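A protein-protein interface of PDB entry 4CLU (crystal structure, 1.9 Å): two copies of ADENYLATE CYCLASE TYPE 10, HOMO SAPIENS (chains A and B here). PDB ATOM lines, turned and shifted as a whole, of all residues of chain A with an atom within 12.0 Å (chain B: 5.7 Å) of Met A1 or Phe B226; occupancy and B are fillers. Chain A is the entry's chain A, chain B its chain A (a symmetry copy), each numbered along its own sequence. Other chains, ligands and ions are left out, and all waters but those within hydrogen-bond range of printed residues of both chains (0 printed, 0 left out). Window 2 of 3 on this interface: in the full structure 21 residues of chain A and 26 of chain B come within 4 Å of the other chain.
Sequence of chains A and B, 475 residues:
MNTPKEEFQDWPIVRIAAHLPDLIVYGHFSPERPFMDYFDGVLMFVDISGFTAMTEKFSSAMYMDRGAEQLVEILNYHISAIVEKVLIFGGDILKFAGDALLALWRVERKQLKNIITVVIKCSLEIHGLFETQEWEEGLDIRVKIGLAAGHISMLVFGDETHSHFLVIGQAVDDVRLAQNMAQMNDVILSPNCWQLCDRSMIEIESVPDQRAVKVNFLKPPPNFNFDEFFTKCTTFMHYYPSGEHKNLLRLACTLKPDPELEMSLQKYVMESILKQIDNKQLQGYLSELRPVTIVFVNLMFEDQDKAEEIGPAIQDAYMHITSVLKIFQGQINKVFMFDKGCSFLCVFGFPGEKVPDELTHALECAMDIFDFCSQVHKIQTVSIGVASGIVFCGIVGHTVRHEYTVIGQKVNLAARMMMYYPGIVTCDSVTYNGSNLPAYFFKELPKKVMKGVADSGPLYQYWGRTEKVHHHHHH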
ATOM      1  N   MET A   1      -3.804  24.840 -23.705  1.00  0.00           N
ATOM      2  CA  MET A   1      -5.023  25.361 -22.912  1.00  0.00           C
ATOM      3  C   MET A   1      -4.685  26.569 -22.104  1.00  0.00           C
ATOM      4  O   MET A   1      -3.764  26.551 -21.321  1.00  0.00           O
ATOM      5  CB  MET A   1      -5.597  24.242 -22.057  1.00  0.00           C
ATOM      6  CG  MET A   1      -6.869  24.494 -21.271  1.00  0.00           C
ATOM      7  SD  MET A   1      -7.939  22.980 -21.064  1.00  0.00           S
ATOM      8  CE  MET A   1      -6.678  21.717 -21.132  1.00  0.00           C
ATOM      9  N   ASN A   2      -5.440  27.651 -22.254  1.00  0.00           N
ATOM     10  CA  ASN A   2      -5.119  28.864 -21.596  1.00  0.00           C
ATOM     11  C   ASN A   2      -5.363  28.884 -20.086  1.00  0.00           C
ATOM     12  O   ASN A   2      -6.191  28.156 -19.579  1.00  0.00           O
ATOM     13  CB  ASN A   2      -5.893  30.055 -22.167  1.00  0.00           C
ATOM     14  CG  ASN A   2      -5.619  30.314 -23.624  1.00  0.00           C
ATOM     15  OD1 ASN A   2      -4.580  29.864 -24.211  1.00  0.00           O
ATOM     16  ND2 ASN A   2      -6.587  30.960 -24.263  1.00  0.00           N
ATOM     17  N   THR A   3      -4.594  29.733 -19.414  1.00  0.00           N
ATOM     18  CA  THR A   3      -4.719  29.987 -17.989  1.00  0.00           C
ATOM     19  C   THR A   3      -4.970  31.468 -17.788  1.00  0.00           C
ATOM     20  O   THR A   3      -4.092  32.215 -17.337  1.00  0.00           O
ATOM     21  CB  THR A   3      -3.477  29.505 -17.200  1.00  0.00           C
ATOM     22  OG1 THR A   3      -2.340  30.243 -17.619  1.00  0.00           O
ATOM     23  CG2 THR A   3      -3.210  28.095 -17.466  1.00  0.00           C
ATOM     24  N   PRO A   4      -6.191  31.913 -18.119  1.00  0.00           N
ATOM     25  CA  PRO A   4      -6.389  33.334 -18.251  1.00  0.00           C
ATOM     26  C   PRO A   4      -6.491  34.037 -16.927  1.00  0.00           C
ATOM     27  O   PRO A   4      -6.677  33.407 -15.903  1.00  0.00           O
ATOM     28  CB  PRO A   4      -7.674  33.453 -19.109  1.00  0.00           C
ATOM     29  CG  PRO A   4      -8.419  32.218 -18.810  1.00  0.00           C
ATOM     30  CD  PRO A   4      -7.372  31.151 -18.566  1.00  0.00           C
ATOM     31  N   LYS A   5      -6.284  35.349 -16.976  1.00  0.00           N
ATOM     32  CA  LYS A   5      -6.294  36.175 -15.775  1.00  0.00           C
ATOM     33  C   LYS A   5      -7.660  35.994 -15.073  1.00  0.00           C
ATOM     34  O   LYS A   5      -8.702  35.981 -15.750  1.00  0.00           O
ATOM     35  CB  LYS A   5      -6.076  37.646 -16.162  1.00  0.00           C
ATOM     36  CG  LYS A   5      -5.211  38.435 -15.179  1.00  0.00           C
ATOM     37  CD  LYS A   5      -5.870  38.682 -13.828  1.00  0.00           C
ATOM     38  CE  LYS A   5      -4.852  38.598 -12.694  1.00  0.00           C
ATOM     39  NZ  LYS A   5      -5.272  39.400 -11.516  1.00  0.00           N
ATOM     40  N   ILE B  88     -12.457  28.183 -21.512  1.00  0.00           N
ATOM     41  CA  ILE B  88     -11.044  27.713 -21.533  1.00  0.00           C
ATOM     42  C   ILE B  88     -10.868  26.453 -22.407  1.00  0.00           C
ATOM     43  O   ILE B  88      -9.829  26.317 -23.041  1.00  0.00           O
ATOM     44  CB  ILE B  88     -10.529  27.503 -20.093  1.00  0.00           C
ATOM     45  CG1 ILE B  88     -10.300  28.884 -19.433  1.00  0.00           C
ATOM     46  CG2 ILE B  88      -9.207  26.704 -20.083  1.00  0.00           C
ATOM     47  CD1 ILE B  88     -10.156  28.809 -17.908  1.00  0.00           C
ATOM     48  N   PHE B  89     -11.873  25.579 -22.448  1.00  0.00           N
ATOM     49  CA  PHE B  89     -11.897  24.366 -23.278  1.00  0.00           C
ATOM     50  C   PHE B  89     -12.352  24.655 -24.699  1.00  0.00           C
ATOM     51  O   PHE B  89     -12.461  23.725 -25.500  1.00  0.00           O
ATOM     52  CB  PHE B  89     -12.771  23.246 -22.651  1.00  0.00           C
ATOM     53  CG  PHE B  89     -12.061  22.452 -21.602  1.00  0.00           C
ATOM     54  CD1 PHE B  89     -11.841  22.974 -20.345  1.00  0.00           C
ATOM     55  CD2 PHE B  89     -11.597  21.178 -21.892  1.00  0.00           C
ATOM     56  CE1 PHE B  89     -11.154  22.269 -19.375  1.00  0.00           C
ATOM     57  CE2 PHE B  89     -10.904  20.449 -20.918  1.00  0.00           C
ATOM     58  CZ  PHE B  89     -10.685  20.993 -19.663  1.00  0.00           C
ATOM     59  N   THR B 117     -13.956  14.411 -27.415  1.00  0.00           N
ATOM     60  CA  THR B 117     -13.079  14.099 -26.262  1.00  0.00           C
ATOM     61  C   THR B 117     -12.790  15.335 -25.407  1.00  0.00           C
ATOM     62  O   THR B 117     -12.808  15.299 -24.181  1.00  0.00           O
ATOM     63  CB  THR B 117     -11.768  13.476 -26.790  1.00  0.00           C
ATOM     64  OG1 THR B 117     -12.143  12.261 -27.416  1.00  0.00           O
ATOM     65  CG2 THR B 117     -10.749  13.201 -25.673  1.00  0.00           C
ATOM     66  N   VAL B 118     -12.523  16.428 -26.091  1.00  0.00           N
ATOM     67  CA  VAL B 118     -12.342  17.745 -25.450  1.00  0.00           C
ATOM     68  C   VAL B 118     -13.551  18.123 -24.585  1.00  0.00           C
ATOM     69  O   VAL B 118     -13.405  18.537 -23.399  1.00  0.00           O
ATOM     70  CB  VAL B 118     -12.065  18.859 -26.501  1.00  0.00           C
ATOM     71  CG1 VAL B 118     -12.114  20.227 -25.869  1.00  0.00           C
ATOM     72  CG2 VAL B 118     -10.715  18.642 -27.155  1.00  0.00           C
ATOM     73  N   LYS B 121     -14.011  15.859 -21.531  1.00  0.00           N
ATOM     74  CA  LYS B 121     -13.051  16.250 -20.517  1.00  0.00           C
ATOM     75  C   LYS B 121     -13.513  17.507 -19.743  1.00  0.00           C
ATOM     76  O   LYS B 121     -13.482  17.578 -18.498  1.00  0.00           O
ATOM     77  CB  LYS B 121     -11.700  16.490 -21.149  1.00  0.00           C
ATOM     78  CG  LYS B 121     -10.594  16.850 -20.179  1.00  0.00           C
ATOM     79  CD  LYS B 121     -10.602  15.877 -19.036  1.00  0.00           C
ATOM     80  CE  LYS B 121      -9.605  16.265 -17.972  1.00  0.00           C
ATOM     81  NZ  LYS B 121      -8.300  15.762 -18.390  1.00  0.00           N
ATOM     82  N   PHE B 224      -0.779   9.232 -24.632  1.00  0.00           N
ATOM     83  CA  PHE B 224      -1.697  10.393 -24.673  1.00  0.00           C
ATOM     84  C   PHE B 224      -1.390  11.487 -23.661  1.00  0.00           C
ATOM     85  O   PHE B 224      -1.144  11.196 -22.500  1.00  0.00           O
ATOM     86  CB  PHE B 224      -3.111   9.919 -24.430  1.00  0.00           C
ATOM     87  CG  PHE B 224      -4.144  10.967 -24.673  1.00  0.00           C
ATOM     88  CD1 PHE B 224      -4.580  11.234 -25.961  1.00  0.00           C
ATOM     89  CD2 PHE B 224      -4.718  11.642 -23.608  1.00  0.00           C
ATOM     90  CE1 PHE B 224      -5.551  12.200 -26.168  1.00  0.00           C
ATOM     91  CE2 PHE B 224      -5.687  12.605 -23.810  1.00  0.00           C
ATOM     92  CZ  PHE B 224      -6.129  12.848 -25.092  1.00  0.00           C
ATOM     93  N   ASN B 225      -1.357  12.746 -24.126  1.00  0.00           N
ATOM     94  CA  ASN B 225      -1.124  13.920 -23.279  1.00  0.00           C
ATOM     95  C   ASN B 225      -2.252  14.908 -23.611  1.00  0.00           C
ATOM     96  O   ASN B 225      -2.346  15.353 -24.750  1.00  0.00           O
ATOM     97  CB  ASN B 225       0.210  14.560 -23.627  1.00  0.00           C
ATOM     98  CG  ASN B 225       0.500  15.775 -22.778  1.00  0.00           C
ATOM     99  OD1 ASN B 225      -0.036  16.860 -22.978  1.00  0.00           O
ATOM    100  ND2 ASN B 225       1.372  15.588 -21.799  1.00  0.00           N
ATOM    101  N   PHE B 226      -3.100  15.228 -22.647  1.00  0.00           N
ATOM    102  CA  PHE B 226      -4.283  16.006 -22.976  1.00  0.00           C
ATOM    103  C   PHE B 226      -3.887  17.425 -23.442  1.00  0.00           C
ATOM    104  O   PHE B 226      -4.473  17.943 -24.371  1.00  0.00           O
ATOM    105  CB  PHE B 226      -5.329  16.039 -21.852  1.00  0.00           C
ATOM    106  CG  PHE B 226      -6.549  16.749 -22.272  1.00  0.00           C
ATOM    107  CD1 PHE B 226      -7.476  16.089 -23.074  1.00  0.00           C
ATOM    108  CD2 PHE B 226      -6.720  18.089 -22.005  1.00  0.00           C
ATOM    109  CE1 PHE B 226      -8.581  16.722 -23.568  1.00  0.00           C
ATOM    110  CE2 PHE B 226      -7.851  18.738 -22.492  1.00  0.00           C
ATOM    111  CZ  PHE B 226      -8.769  18.048 -23.300  1.00  0.00           C
ATOM    112  N   ASP B 227      -2.873  18.044 -22.838  1.00  0.00           N
ATOM    113  CA  ASP B 227      -2.487  19.386 -23.265  1.00  0.00           C
ATOM    114  C   ASP B 227      -2.025  19.409 -24.718  1.00  0.00           C
ATOM    115  O   ASP B 227      -2.361  20.307 -25.462  1.00  0.00           O
ATOM    116  CB  ASP B 227      -1.364  19.921 -22.409  1.00  0.00           C
ATOM    117  CG  ASP B 227      -1.750  20.079 -20.960  1.00  0.00           C
ATOM    118  OD1 ASP B 227      -2.959  20.088 -20.604  1.00  0.00           O
ATOM    119  OD2 ASP B 227      -0.788  20.142 -20.163  1.00  0.00           O
ATOM    120  N   GLU B 228      -1.223  18.432 -25.117  1.00  0.00           N
ATOM    121  CA  GLU B 228      -0.789  18.348 -26.498  1.00  0.00           C
ATOM    122  C   GLU B 228      -1.954  18.076 -27.441  1.00  0.00           C
ATOM    123  O   GLU B 228      -2.049  18.706 -28.501  1.00  0.00           O
ATOM    124  CB  GLU B 228       0.301  17.281 -26.676  1.00  0.00           C
ATOM    125  CG  GLU B 228       1.550  17.680 -25.918  1.00  0.00           C
ATOM    126  CD  GLU B 228       2.654  16.656 -25.970  1.00  0.00           C
ATOM    127  OE1 GLU B 228       2.412  15.471 -26.344  1.00  0.00           O
ATOM    128  OE2 GLU B 228       3.763  17.091 -25.632  1.00  0.00           O
ATOM    129  N   PHE B 229      -2.857  17.176 -27.039  1.00  0.00           N
ATOM    130  CA  PHE B 229      -4.074  16.895 -27.789  1.00  0.00           C
ATOM    131  C   PHE B 229      -4.933  18.166 -27.948  1.00  0.00           C
ATOM    132  O   PHE B 229      -5.418  18.512 -29.026  1.00  0.00           O
ATOM    133  CB  PHE B 229      -4.843  15.831 -27.048  1.00  0.00           C
ATOM    134  CG  PHE B 229      -6.111  15.462 -27.686  1.00  0.00           C
ATOM    135  CD1 PHE B 229      -6.115  14.782 -28.852  1.00  0.00           C
ATOM    136  CD2 PHE B 229      -7.311  15.845 -27.122  1.00  0.00           C
ATOM    137  CE1 PHE B 229      -7.296  14.432 -29.451  1.00  0.00           C
ATOM    138  CE2 PHE B 229      -8.500  15.564 -27.750  1.00  0.00           C
ATOM    139  CZ  PHE B 229      -8.496  14.827 -28.899  1.00  0.00           C
ATOM    140  N   PHE B 230      -5.190  18.815 -26.843  1.00  0.00           N
ATOM    141  CA  PHE B 230      -5.969  20.070 -26.869  1.00  0.00           C
ATOM    142  C   PHE B 230      -5.341  21.052 -27.825  1.00  0.00           C
ATOM    143  O   PHE B 230      -6.029  21.689 -28.662  1.00  0.00           O
ATOM    144  CB  PHE B 230      -6.065  20.648 -25.481  1.00  0.00           C
ATOM    145  CG  PHE B 230      -6.947  21.845 -25.414  1.00  0.00           C
ATOM    146  CD1 PHE B 230      -8.347  21.693 -25.345  1.00  0.00           C
ATOM    147  CD2 PHE B 230      -6.399  23.119 -25.474  1.00  0.00           C
ATOM    148  CE1 PHE B 230      -9.166  22.821 -25.341  1.00  0.00           C
ATOM    149  CE2 PHE B 230      -7.205  24.228 -25.506  1.00  0.00           C
ATOM    150  CZ  PHE B 230      -8.597  24.093 -25.427  1.00  0.00           C
ATOM    151  N   THR B 231      -4.029  21.219 -27.720  1.00  0.00           N
ATOM    152  CA  THR B 231      -3.350  22.129 -28.617  1.00  0.00           C
ATOM    153  C   THR B 231      -3.635  21.809 -30.103  1.00  0.00           C
ATOM    154  O   THR B 231      -3.955  22.758 -30.867  1.00  0.00           O
ATOM    155  CB  THR B 231      -1.851  22.193 -28.360  1.00  0.00           C
ATOM    156  OG1 THR B 231      -1.654  22.689 -27.047  1.00  0.00           O
ATOM    157  CG2 THR B 231      -1.206  23.145 -29.342  1.00  0.00           C
ATOM    158  N   TYR B 240     -10.279  30.914 -30.577  1.00  0.00           N
ATOM    159  CA  TYR B 240      -9.554  30.636 -29.347  1.00  0.00           C
ATOM    160  C   TYR B 240      -8.514  31.732 -29.010  1.00  0.00           C
ATOM    161  O   TYR B 240      -7.593  32.001 -29.798  1.00  0.00           O
ATOM    162  CB  TYR B 240      -8.872  29.259 -29.361  1.00  0.00           C
ATOM    163  CG  TYR B 240      -8.573  28.778 -27.964  1.00  0.00           C
ATOM    164  CD1 TYR B 240      -9.602  28.465 -27.086  1.00  0.00           C
ATOM    165  CD2 TYR B 240      -7.293  28.586 -27.528  1.00  0.00           C
ATOM    166  CE1 TYR B 240      -9.320  28.020 -25.806  1.00  0.00           C
ATOM    167  CE2 TYR B 240      -7.023  28.166 -26.266  1.00  0.00           C
ATOM    168  CZ  TYR B 240      -8.017  27.860 -25.409  1.00  0.00           C
ATOM    169  OH  TYR B 240      -7.734  27.443 -24.118  1.00  0.00           O
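Ile B88 touches Met A1.
Met A1 touches Phe B89 (SD to CZ, 3.7 Å).
Met A1 touches Phe B226 (CE to CE2, 3.5 Å).
Phe B230 touches Met A1 (CE2 to CA, 3.6 Å).
Met A1 touches Tyr B240.
O of Asn A2 touches CG2 of Ile B88, at 3.4 Å.
Ile B88 touches Pro A4 (CD1 to CD, 3.7 Å).
No position is printed for both chains.
Printed residues of chain B within 4 Å of Met A1: Ile B88, Phe B89, Phe B226, Phe B230 and Tyr B240.
Phe B226 touches one residue of chain A.
Of chain A, only Met A1 (3.4 Å), Asn A2 (3.4 Å) and Pro A4 (3.7 Å) come within 4 Å of Ile B88.
No residue of chain A comes within 4 Å of Thr B117.
No residue of chain A comes within 4 Å of Lys B121.
No residue of chain A comes within 4 Å of Phe B224.
Glu B228 touches none of the printed residues of chain A.
Phe B230 touches just one residue of chain A: Met A1 (3.6 Å).
No residue of chain A comes within 4 Å of Thr B231.
Of the printed residues of chain B, Pro A4 touches Ile B88 (3.7 Å).
Printed residues of chain A within 4 Å of Tyr B240: Met A1 and Asn A2.
Printed residues of chain B within 4 Å of Asn A2: Ile B88 and Tyr B240.
The nearest printed residue of chain A that does not touch Tyr B240 is Thr A3 (6.1 Å).
The backbone carbonyl oxygen (O) of Ile B88 lies within hydrogen-bond range of the side-chain hydroxyl (OH) of Tyr B240, at 2.6 Å.
OH of Tyr B240 lies within hydrogen-bond range of N of Asn A2.
Hydrophobic or aromatic side chains of chain A within 4 Å of the printed part of chain B: Met A1 and Pro A4.
Printed residues of chain B that touch a printed residue of chain A: Ile B88, Phe B89, Phe B226, Phe B230 and Tyr B240.
Hydrophobic or aromatic side chains of chain B that line the printed part of chain A: Ile B88, Phe B89, Phe B226, Phe B230 and Tyr B240.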
